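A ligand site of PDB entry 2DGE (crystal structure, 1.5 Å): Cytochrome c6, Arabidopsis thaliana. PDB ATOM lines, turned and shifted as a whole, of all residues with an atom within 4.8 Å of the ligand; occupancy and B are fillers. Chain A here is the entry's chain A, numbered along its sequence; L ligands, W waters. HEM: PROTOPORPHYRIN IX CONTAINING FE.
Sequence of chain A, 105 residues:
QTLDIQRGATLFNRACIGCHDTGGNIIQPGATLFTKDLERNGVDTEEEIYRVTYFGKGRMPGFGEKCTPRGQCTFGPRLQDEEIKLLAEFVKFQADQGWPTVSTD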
ATOM      1  N   PHE A  12     -34.606  21.179  13.409  1.00  0.00           N
ATOM      2  CA  PHE A  12     -33.487  20.745  14.249  1.00  0.00           C
ATOM      3  C   PHE A  12     -33.960  20.524  15.681  1.00  0.00           C
ATOM      4  O   PHE A  12     -33.567  19.540  16.331  1.00  0.00           O
ATOM      5  CB  PHE A  12     -32.361  21.793  14.206  1.00  0.00           C
ATOM      6  CG  PHE A  12     -31.095  21.365  14.934  1.00  0.00           C
ATOM      7  CD1 PHE A  12     -30.091  20.694  14.251  1.00  0.00           C
ATOM      8  CD2 PHE A  12     -30.906  21.688  16.275  1.00  0.00           C
ATOM      9  CE1 PHE A  12     -28.900  20.317  14.905  1.00  0.00           C
ATOM     10  CE2 PHE A  12     -29.730  21.298  16.928  1.00  0.00           C
ATOM     11  CZ  PHE A  12     -28.741  20.614  16.243  1.00  0.00           C
ATOM     12  N   ALA A  15     -35.966  17.176  15.664  1.00  0.00           N
ATOM     13  CA  ALA A  15     -35.354  15.900  15.282  1.00  0.00           C
ATOM     14  C   ALA A  15     -33.958  15.629  15.844  1.00  0.00           C
ATOM     15  O   ALA A  15     -33.531  14.472  15.891  1.00  0.00           O
ATOM     16  CB  ALA A  15     -35.333  15.763  13.768  1.00  0.00           C
ATOM     17  N   CYS A  16     -33.234  16.665  16.229  1.00  0.00           N
ATOM     18  CA  CYS A  16     -31.786  16.521  16.442  1.00  0.00           C
ATOM     19  C   CYS A  16     -31.336  16.885  17.844  1.00  0.00           C
ATOM     20  O   CYS A  16     -30.191  16.634  18.231  1.00  0.00           O
ATOM     21  CB  CYS A  16     -31.015  17.363  15.427  1.00  0.00           C
ATOM     22  SG  CYS A  16     -31.564  17.178  13.704  1.00  0.00           S
ATOM     23  N   CYS A  19     -29.423  14.667  20.779  1.00  0.00           N
ATOM     24  CA  CYS A  19     -27.999  14.438  20.873  1.00  0.00           C
ATOM     25  C   CYS A  19     -27.161  15.680  20.584  1.00  0.00           C
ATOM     26  O   CYS A  19     -26.028  15.765  21.049  1.00  0.00           O
ATOM     27  CB  CYS A  19     -27.574  13.293  19.955  1.00  0.00           C
ATOM     28  SG  CYS A  19     -28.431  11.727  20.288  1.00  0.00           S
ATOM     29  N   HIS A  20     -27.722  16.639  19.844  1.00  0.00           N
ATOM     30  CA  HIS A  20     -26.934  17.772  19.353  1.00  0.00           C
ATOM     31  C   HIS A  20     -27.436  19.143  19.834  1.00  0.00           C
ATOM     32  O   HIS A  20     -27.224  20.153  19.167  1.00  0.00           O
ATOM     33  CB  HIS A  20     -26.916  17.769  17.802  1.00  0.00           C
ATOM     34  CG  HIS A  20     -26.261  16.573  17.167  1.00  0.00           C
ATOM     35  ND1 HIS A  20     -24.937  16.234  17.361  1.00  0.00           N
ATOM     36  CD2 HIS A  20     -26.759  15.655  16.299  1.00  0.00           C
ATOM     37  CE1 HIS A  20     -24.650  15.160  16.634  1.00  0.00           C
ATOM     38  NE2 HIS A  20     -25.734  14.800  15.967  1.00  0.00           N
ATOM     39  N   ASN A  25     -22.546  17.182  21.131  1.00  0.00           N
ATOM     40  CA  ASN A  25     -22.788  15.760  20.877  1.00  0.00           C
ATOM     41  C   ASN A  25     -22.675  15.033  22.214  1.00  0.00           C
ATOM     42  O   ASN A  25     -21.570  14.849  22.740  1.00  0.00           O
ATOM     43  CB  ASN A  25     -21.811  15.202  19.834  1.00  0.00           C
ATOM     44  CG  ASN A  25     -22.180  13.778  19.371  1.00  0.00           C
ATOM     45  OD1 ASN A  25     -22.753  13.004  20.130  1.00  0.00           O
ATOM     46  ND2 ASN A  25     -21.842  13.441  18.131  1.00  0.00           N
ATOM     47  N   ILE A  27     -23.347  11.904  22.845  1.00  0.00           N
ATOM     48  CA  ILE A  27     -23.103  10.478  22.754  1.00  0.00           C
ATOM     49  C   ILE A  27     -21.635  10.160  22.907  1.00  0.00           C
ATOM     50  O   ILE A  27     -21.262   9.252  23.657  1.00  0.00           O
ATOM     51  CB  ILE A  27     -23.683   9.886  21.450  1.00  0.00           C
ATOM     52  CG1 ILE A  27     -25.212  10.030  21.439  1.00  0.00           C
ATOM     53  CG2 ILE A  27     -23.252   8.434  21.253  1.00  0.00           C
ATOM     54  CD1 ILE A  27     -25.927   9.444  22.684  1.00  0.00           C
ATOM     55  N   GLN A  28     -20.794  10.906  22.192  1.00  0.00           N
ATOM     56  CA  GLN A  28     -19.363  10.634  22.149  1.00  0.00           C
ATOM     57  C   GLN A  28     -18.591  11.920  21.907  1.00  0.00           C
ATOM     58  O   GLN A  28     -19.114  12.868  21.296  1.00  0.00           O
ATOM     59  CB  GLN A  28     -19.037   9.625  21.047  1.00  0.00           C
ATOM     60  CG  GLN A  28     -19.404  10.068  19.643  1.00  0.00           C
ATOM     61  CD  GLN A  28     -19.131   8.993  18.604  1.00  0.00           C
ATOM     62  OE1 GLN A  28     -18.279   9.178  17.726  1.00  0.00           O
ATOM     63  NE2 GLN A  28     -19.849   7.889  18.705  1.00  0.00           N
ATOM     64  N   GLY A  30     -15.627  14.539  20.430  1.00  0.00           N
ATOM     65  CA  GLY A  30     -14.966  14.831  19.174  1.00  0.00           C
ATOM     66  C   GLY A  30     -15.831  14.793  17.935  1.00  0.00           C
ATOM     67  O   GLY A  30     -15.315  14.761  16.827  1.00  0.00           O
ATOM     68  N   ALA A  31     -17.146  14.805  18.108  1.00  0.00           N
ATOM     69  CA  ALA A  31     -18.048  14.724  16.966  1.00  0.00           C
ATOM     70  C   ALA A  31     -19.218  15.689  17.121  1.00  0.00           C
ATOM     71  O   ALA A  31     -20.369  15.346  16.819  1.00  0.00           O
ATOM     72  CB  ALA A  31     -18.553  13.283  16.775  1.00  0.00           C
ATOM     73  N   THR A  32     -18.916  16.911  17.583  1.00  0.00           N
ATOM     74  CA  THR A  32     -19.939  17.954  17.694  1.00  0.00           C
ATOM     75  C   THR A  32     -20.230  18.523  16.313  1.00  0.00           C
ATOM     76  O   THR A  32     -19.596  18.167  15.328  1.00  0.00           O
ATOM     77  CB  THR A  32     -19.503  19.114  18.621  1.00  0.00           C
ATOM     78  OG1 THR A  32     -18.434  19.844  18.000  1.00  0.00           O
ATOM     79  CG2 THR A  32     -18.955  18.583  19.962  1.00  0.00           C
ATOM     80  N   LEU A  33     -21.165  19.461  16.270  1.00  0.00           N
ATOM     81  CA  LEU A  33     -21.497  20.098  15.017  1.00  0.00           C
ATOM     82  C   LEU A  33     -20.735  21.422  14.830  1.00  0.00           C
ATOM     83  O   LEU A  33     -21.079  22.213  13.946  1.00  0.00           O
ATOM     84  CB  LEU A  33     -23.008  20.306  14.923  1.00  0.00           C
ATOM     85  CG  LEU A  33     -23.901  19.084  15.204  1.00  0.00           C
ATOM     86  CD1 LEU A  33     -25.362  19.422  14.932  1.00  0.00           C
ATOM     87  CD2 LEU A  33     -23.470  17.894  14.372  1.00  0.00           C
ATOM     88  N   ASP A  37     -14.800  20.008  14.581  1.00  0.00           N
ATOM     89  CA  ASP A  37     -15.155  18.588  14.601  1.00  0.00           C
ATOM     90  C   ASP A  37     -15.699  18.113  13.249  1.00  0.00           C
ATOM     91  O   ASP A  37     -15.386  17.015  12.781  1.00  0.00           O
ATOM     92  CB  ASP A  37     -16.141  18.274  15.729  1.00  0.00           C
ATOM     93  CG  ASP A  37     -15.495  18.281  17.108  1.00  0.00           C
ATOM     94  OD1 ASP A  37     -16.244  18.196  18.106  1.00  0.00           O
ATOM     95  OD2 ASP A  37     -14.261  18.381  17.281  1.00  0.00           O
ATOM     96  N   LEU A  38     -16.502  18.949  12.589  1.00  0.00           N
ATOM     97  CA  LEU A  38     -16.935  18.607  11.230  1.00  0.00           C
ATOM     98  C   LEU A  38     -15.718  18.405  10.323  1.00  0.00           C
ATOM     99  O   LEU A  38     -15.684  17.468   9.525  1.00  0.00           O
ATOM    100  CB  LEU A  38     -17.834  19.705  10.661  1.00  0.00           C
ATOM    101  CG  LEU A  38     -19.197  19.930  11.351  1.00  0.00           C
ATOM    102  CD1 LEU A  38     -19.918  21.079  10.633  1.00  0.00           C
ATOM    103  CD2 LEU A  38     -20.078  18.669  11.386  1.00  0.00           C
ATOM    104  N   ASN A  41     -13.692  15.207  11.216  1.00  0.00           N
ATOM    105  CA  ASN A  41     -14.368  13.973  10.839  1.00  0.00           C
ATOM    106  C   ASN A  41     -14.657  13.862   9.342  1.00  0.00           C
ATOM    107  O   ASN A  41     -15.147  12.835   8.874  1.00  0.00           O
ATOM    108  CB  ASN A  41     -15.675  13.824  11.628  1.00  0.00           C
ATOM    109  CG  ASN A  41     -15.455  13.475  13.085  1.00  0.00           C
ATOM    110  OD1 ASN A  41     -15.573  14.331  13.976  1.00  0.00           O
ATOM    111  ND2 ASN A  41     -15.167  12.214  13.344  1.00  0.00           N
ATOM    112  N   VAL A  43     -16.876  15.686   7.717  1.00  0.00           N
ATOM    113  CA  VAL A  43     -18.305  15.979   7.499  1.00  0.00           C
ATOM    114  C   VAL A  43     -18.516  17.501   7.460  1.00  0.00           C
ATOM    115  O   VAL A  43     -19.359  18.055   8.178  1.00  0.00           O
ATOM    116  CB  VAL A  43     -19.208  15.320   8.578  1.00  0.00           C
ATOM    117  CG1 VAL A  43     -20.694  15.402   8.187  1.00  0.00           C
ATOM    118  CG2 VAL A  43     -18.795  13.865   8.813  1.00  0.00           C
ATOM    119  N   ILE A  49     -22.939  16.350   5.178  1.00  0.00           N
ATOM    120  CA  ILE A  49     -23.867  16.547   6.290  1.00  0.00           C
ATOM    121  C   ILE A  49     -25.222  15.923   5.910  1.00  0.00           C
ATOM    122  O   ILE A  49     -25.829  15.232   6.719  1.00  0.00           O
ATOM    123  CB  ILE A  49     -24.026  18.048   6.670  1.00  0.00           C
ATOM    124  CG1 ILE A  49     -22.734  18.616   7.286  1.00  0.00           C
ATOM    125  CG2 ILE A  49     -25.156  18.248   7.655  1.00  0.00           C
ATOM    126  CD1 ILE A  49     -22.633  20.147   7.172  1.00  0.00           C
ATOM    127  N   VAL A  52     -24.826  11.983   6.033  1.00  0.00           N
ATOM    128  CA  VAL A  52     -24.812  11.496   7.408  1.00  0.00           C
ATOM    129  C   VAL A  52     -26.226  11.556   8.010  1.00  0.00           C
ATOM    130  O   VAL A  52     -26.682  10.606   8.646  1.00  0.00           O
ATOM    131  CB  VAL A  52     -23.778  12.289   8.264  1.00  0.00           C
ATOM    132  CG1 VAL A  52     -23.985  12.087   9.764  1.00  0.00           C
ATOM    133  CG2 VAL A  52     -22.341  11.951   7.842  1.00  0.00           C
ATOM    134  N   THR A  53     -26.939  12.664   7.791  1.00  0.00           N
ATOM    135  CA  THR A  53     -28.291  12.798   8.320  1.00  0.00           C
ATOM    136  C   THR A  53     -29.272  11.812   7.683  1.00  0.00           C
ATOM    137  O   THR A  53     -30.158  11.294   8.374  1.00  0.00           O
ATOM    138  CB  THR A  53     -28.790  14.243   8.115  1.00  0.00           C
ATOM    139  OG1 THR A  53     -27.873  15.151   8.734  1.00  0.00           O
ATOM    140  CG2 THR A  53     -30.078  14.482   8.866  1.00  0.00           C
ATOM    141  N   LYS A  57     -24.789   7.182  10.674  1.00  0.00           N
ATOM    142  CA  LYS A  57     -23.357   6.956  10.798  1.00  0.00           C
ATOM    143  C   LYS A  57     -23.044   6.467  12.208  1.00  0.00           C
ATOM    144  O   LYS A  57     -23.249   7.186  13.186  1.00  0.00           O
ATOM    145  CB  LYS A  57     -22.599   8.263  10.508  1.00  0.00           C
ATOM    146  CG  LYS A  57     -21.089   8.189  10.677  1.00  0.00           C
ATOM    147  CD  LYS A  57     -20.412   9.334   9.968  1.00  0.00           C
ATOM    148  CE  LYS A  57     -18.909   9.199  10.050  1.00  0.00           C
ATOM    149  NZ  LYS A  57     -18.216  10.491   9.760  1.00  0.00           N
ATOM    150  N   GLY A  58     -22.573   5.237  12.306  1.00  0.00           N
ATOM    151  CA  GLY A  58     -22.233   4.679  13.608  1.00  0.00           C
ATOM    152  C   GLY A  58     -23.397   4.735  14.568  1.00  0.00           C
ATOM    153  O   GLY A  58     -24.491   4.228  14.277  1.00  0.00           O
ATOM    154  N   ARG A  59     -23.183   5.407  15.695  1.00  0.00           N
ATOM    155  CA  ARG A  59     -24.184   5.508  16.758  1.00  0.00           C
ATOM    156  C   ARG A  59     -25.289   6.531  16.466  1.00  0.00           C
ATOM    157  O   ARG A  59     -26.231   6.664  17.250  1.00  0.00           O
ATOM    158  CB  ARG A  59     -23.493   5.809  18.089  1.00  0.00           C
ATOM    159  CG  ARG A  59     -22.783   4.578  18.646  1.00  0.00           C
ATOM    160  CD  ARG A  59     -22.019   4.828  19.930  1.00  0.00           C
ATOM    161  NE  ARG A  59     -21.296   3.626  20.339  1.00  0.00           N
ATOM    162  CZ  ARG A  59     -20.001   3.394  20.102  1.00  0.00           C
ATOM    163  NH1 ARG A  59     -19.456   2.266  20.513  1.00  0.00           N
ATOM    164  NH2 ARG A  59     -19.258   4.296  19.476  1.00  0.00           N
ATOM    165  N   MET A  60     -25.172   7.228  15.344  1.00  0.00           N
ATOM    166  CA  MET A  60     -26.211   8.155  14.889  1.00  0.00           C
ATOM    167  C   MET A  60     -27.169   7.452  13.930  1.00  0.00           C
ATOM    168  O   MET A  60     -26.741   6.956  12.893  1.00  0.00           O
ATOM    169  CB  MET A  60     -25.609   9.347  14.146  1.00  0.00           C
ATOM    170  CG  MET A  60     -26.693  10.273  13.611  1.00  0.00           C
ATOM    171  SD  MET A  60     -26.047  11.778  12.962  1.00  0.00           S
ATOM    172  CE  MET A  60     -27.330  12.086  11.708  1.00  0.00           C
ATOM    173  N   PRO A  61     -28.459   7.468  14.244  1.00  0.00           N
ATOM    174  CA  PRO A  61     -29.454   6.899  13.331  1.00  0.00           C
ATOM    175  C   PRO A  61     -29.650   7.779  12.103  1.00  0.00           C
ATOM    176  O   PRO A  61     -29.480   8.989  12.194  1.00  0.00           O
ATOM    177  CB  PRO A  61     -30.742   6.864  14.173  1.00  0.00           C
ATOM    178  CG  PRO A  61     -30.521   7.774  15.346  1.00  0.00           C
ATOM    179  CD  PRO A  61     -29.056   8.009  15.470  1.00  0.00           C
ATOM    180  N   PHE A  63     -32.128   9.324   9.052  1.00  0.00           N
ATOM    181  CA  PHE A  63     -33.480   9.866   9.043  1.00  0.00           C
ATOM    182  C   PHE A  63     -34.122   9.824   7.659  1.00  0.00           C
ATOM    183  O   PHE A  63     -35.296  10.166   7.504  1.00  0.00           O
ATOM    184  CB  PHE A  63     -33.472  11.290   9.602  1.00  0.00           C
ATOM    185  CG  PHE A  63     -33.215  11.362  11.085  1.00  0.00           C
ATOM    186  CD1 PHE A  63     -31.904  11.278  11.579  1.00  0.00           C
ATOM    187  CD2 PHE A  63     -34.267  11.507  11.983  1.00  0.00           C
ATOM    188  CE1 PHE A  63     -31.659  11.327  12.959  1.00  0.00           C
ATOM    189  CE2 PHE A  63     -34.029  11.565  13.354  1.00  0.00           C
ATOM    190  CZ  PHE A  63     -32.717  11.482  13.838  1.00  0.00           C
ATOM    191  N   LEU A  79     -37.700  11.746   7.877  1.00  0.00           N
ATOM    192  CA  LEU A  79     -37.788  13.103   7.354  1.00  0.00           C
ATOM    193  C   LEU A  79     -37.814  13.086   5.823  1.00  0.00           C
ATOM    194  O   LEU A  79     -37.245  12.197   5.203  1.00  0.00           O
ATOM    195  CB  LEU A  79     -36.610  13.943   7.861  1.00  0.00           C
ATOM    196  CG  LEU A  79     -36.551  14.188   9.366  1.00  0.00           C
ATOM    197  CD1 LEU A  79     -35.193  14.760   9.761  1.00  0.00           C
ATOM    198  CD2 LEU A  79     -37.667  15.105   9.847  1.00  0.00           C
ATOM    199  N   LEU A  87     -31.946  20.898   6.947  1.00  0.00           N
ATOM    200  CA  LEU A  87     -31.121  20.569   8.115  1.00  0.00           C
ATOM    201  C   LEU A  87     -29.632  20.642   7.808  1.00  0.00           C
ATOM    202  O   LEU A  87     -28.858  21.140   8.636  1.00  0.00           O
ATOM    203  CB  LEU A  87     -31.502  19.192   8.673  1.00  0.00           C
ATOM    204  CG  LEU A  87     -32.752  19.266   9.536  1.00  0.00           C
ATOM    205  CD1 LEU A  87     -33.351  17.877   9.664  1.00  0.00           C
ATOM    206  CD2 LEU A  87     -32.514  19.902  10.911  1.00  0.00           C
ATOM    207  N   VAL A  91     -27.102  23.172   9.719  1.00  0.00           N
ATOM    208  CA  VAL A  91     -25.863  22.768  10.389  1.00  0.00           C
ATOM    209  C   VAL A  91     -24.638  23.480   9.805  1.00  0.00           C
ATOM    210  O   VAL A  91     -23.796  23.967  10.550  1.00  0.00           O
ATOM    211  CB  VAL A  91     -25.697  21.244  10.349  1.00  0.00           C
ATOM    212  CG1 VAL A  91     -24.321  20.831  10.856  1.00  0.00           C
ATOM    213  CG2 VAL A  91     -26.770  20.577  11.178  1.00  0.00           C
HETATM  214  CHA HEM L   1     -22.628  13.033  13.933  1.00  0.00           C
HETATM  215  CHB HEM L   1     -26.146  15.814  12.181  1.00  0.00           C
HETATM  216  CHC HEM L   1     -29.378  13.490  14.974  1.00  0.00           C
HETATM  217  CHD HEM L   1     -25.696  11.307  17.261  1.00  0.00           C
HETATM  218  C1A HEM L   1     -23.315  13.996  13.255  1.00  0.00           C
HETATM  219  C2A HEM L   1     -22.701  14.895  12.308  1.00  0.00           C
HETATM  220  C3A HEM L   1     -23.682  15.678  11.816  1.00  0.00           C
HETATM  221  C4A HEM L   1     -24.924  15.265  12.424  1.00  0.00           C
HETATM  222  CMA HEM L   1     -23.562  16.802  10.771  1.00  0.00           C
HETATM  223  CAA HEM L   1     -21.192  14.945  11.998  1.00  0.00           C
HETATM  224  CBA HEM L   1     -20.515  15.617  13.209  1.00  0.00           C
HETATM  225  CGA HEM L   1     -19.012  15.484  13.272  1.00  0.00           C
HETATM  226  O1A HEM L   1     -18.458  14.636  12.536  1.00  0.00           O
HETATM  227  O2A HEM L   1     -18.355  16.219  14.047  1.00  0.00           O
HETATM  228  C1B HEM L   1     -27.329  15.425  12.781  1.00  0.00           C
HETATM  229  C2B HEM L   1     -28.623  15.986  12.490  1.00  0.00           C
HETATM  230  C3B HEM L   1     -29.530  15.361  13.261  1.00  0.00           C
HETATM  231  C4B HEM L   1     -28.822  14.362  14.055  1.00  0.00           C
HETATM  232  CMB HEM L   1     -28.826  17.137  11.464  1.00  0.00           C
HETATM  233  CAB HEM L   1     -31.054  15.637  13.275  1.00  0.00           C
HETATM  234  CBB HEM L   1     -31.749  15.128  12.223  1.00  0.00           C
HETATM  235  C1C HEM L   1     -28.630  12.761  15.878  1.00  0.00           C
HETATM  236  C2C HEM L   1     -29.148  12.100  17.050  1.00  0.00           C
HETATM  237  C3C HEM L   1     -28.140  11.491  17.692  1.00  0.00           C
HETATM  238  C4C HEM L   1     -26.946  11.741  16.916  1.00  0.00           C
HETATM  239  CMC HEM L   1     -30.627  12.119  17.428  1.00  0.00           C
HETATM  240  CAC HEM L   1     -28.249  10.671  19.012  1.00  0.00           C
HETATM  241  CBC HEM L   1     -28.851   9.455  18.997  1.00  0.00           C
HETATM  242  C1D HEM L   1     -24.570  11.496  16.510  1.00  0.00           C
HETATM  243  C2D HEM L   1     -23.345  10.748  16.680  1.00  0.00           C
HETATM  244  C3D HEM L   1     -22.368  11.267  15.645  1.00  0.00           C
HETATM  245  C4D HEM L   1     -23.121  12.295  14.946  1.00  0.00           C
HETATM  246  CMD HEM L   1     -23.082   9.634  17.710  1.00  0.00           C
HETATM  247  CAD HEM L   1     -20.933  10.773  15.407  1.00  0.00           C
HETATM  248  CBD HEM L   1     -21.021   9.748  14.269  1.00  0.00           C
HETATM  249  CGD HEM L   1     -19.665   9.185  13.935  1.00  0.00           C
HETATM  250  O1D HEM L   1     -18.803   9.950  13.422  1.00  0.00           O
HETATM  251  O2D HEM L   1     -19.459   7.968  14.129  1.00  0.00           O
HETATM  252  NA  HEM L   1     -24.671  14.225  13.311  1.00  0.00           N
HETATM  253  NB  HEM L   1     -27.483  14.428  13.730  1.00  0.00           N
HETATM  254  NC  HEM L   1     -27.265  12.554  15.813  1.00  0.00           N
HETATM  255  ND  HEM L   1     -24.407  12.382  15.458  1.00  0.00           N
HETATM  256 FE   HEM L   1     -25.952  13.406  14.589  1.00  0.00          FE
HETATM  257  O   HOH W   1     -19.063  11.997  11.891  1.00  0.00           O
HETATM  258  O   HOH W   2     -16.305   9.897  12.401  1.00  0.00           O
HETATM  259  O   HOH W   3     -20.675   6.664  16.268  1.00  0.00           O
HETATM  260  O   HOH W   4     -33.124  13.977  18.527  1.00  0.00           O
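SD of Met 60 is bound to FE of the ligand, 2.3 Å away.
A carbon (CAC) of the ligand is covalently linked to the side-chain sulfur of Cys 19 (1.7 Å).
A carbon (CAB) of the ligand is covalently linked to the side-chain sulfur (SG) of Cys 16 (1.7 Å).
The side-chain amino group (NZ) of Lys 57 is in salt-bridge range of an oxygen (O1D) of the ligand.
The side-chain amide oxygen (OD1) of Asn 41 sits close to an oxygen (O1A) of the ligand, 3.2 Å away.
O of Thr 32 lies close to O2A of the ligand (2.6 Å).
NE2 of His 20 is bound to FE of the ligand (2.0 Å).
N of Leu 79 sits at hydrogen-bond distance from O of Phe 63 (2.9 Å).
The backbone carbonyl oxygen of Thr 53 lies within hydrogen-bond range of the backbone NH of Phe 63 (2.9 Å).
The side-chain amide oxygen (OD1) of Asn 41 sits close to the backbone carbonyl oxygen (O) of Gly 30.
O of Ile 49 sits at hydrogen-bond distance from OG1 of Thr 53.
The backbone carbonyl oxygen (O) of Ala 31 is in hydrogen-bond range of the side-chain amide nitrogen (ND2) of Asn 25 (2.7 Å).
N of Ile 27 sits at hydrogen-bond distance from OD1 of Asn 25, at 3.0 Å.
O of Leu 38 lies within hydrogen-bond range of N of Val 43 (2.8 Å).
The side-chain hydroxyl (OG1) of Thr 32 is in hydrogen-bond range of the side-chain carboxylate (OD1) of Asp 37 (2.7 Å).
O of Asp 37 sits close to O2A of the ligand, at 3.3 Å.
O of Ala 15 touches CAB of the ligand, at 3.8 Å.
Asn 25 touches the ligand (ND2 to C3D, 3.3 Å).
Ile 27 touches the ligand (CG2 to CMD, 3.7 Å).
Gln 28 touches the ligand (NE2 to CMD, 3.8 Å).
Ala 31 touches the ligand.
Leu 33 touches the ligand.
Leu 38 touches the ligand (CD2 to CBA, 3.6 Å).
CG2 of Val 43 touches O1A of the ligand (3.8 Å).
CG2 of Ile 49 touches CMA of the ligand, 3.8 Å away.
Thr 53 touches the ligand (OG1 to CMB, 3.5 Å).
Arg 59 touches the ligand (CB to CMD, 3.9 Å).
Pro 61 touches the ligand.
CE1 of Phe 63 touches CHC of the ligand (3.7 Å).
Hydrophobic or aromatic side chains within 4 Å of the ligand: Ala 15, His 20, Ile 27, Ala 31, Leu 33, Leu 38, Val 43, Ile 49, Met 60, Pro 61 and Phe 63.
21 residues have an atom within 4 Å of the ligand: Ala 15, Cys 16, Cys 19, His 20, Asn 25, Ile 27, Gln 28, Ala 31, Thr 32, Leu 33, Asp 37, Leu 38, Asn 41, Val 43, Ile 49, Thr 53, Lys 57, Arg 59, Met 60, Pro 61 and Phe 63.
Water W1 bridges O1D of the ligand and NZ of Lys 57.
Water W2 lies within hydrogen-bond range of O1D of the ligand (2.7 Å), ND2 of Asn 41 (2.7 Å) and NZ of Lys 57 (3.3 Å).
Water W3 lies within hydrogen-bond range of an oxygen (O2D) of the ligand (2.8 Å), the side-chain amide nitrogen (NE2) of Gln 28 (2.8 Å) and the backbone NH (N) of Arg 59 (2.9 Å).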
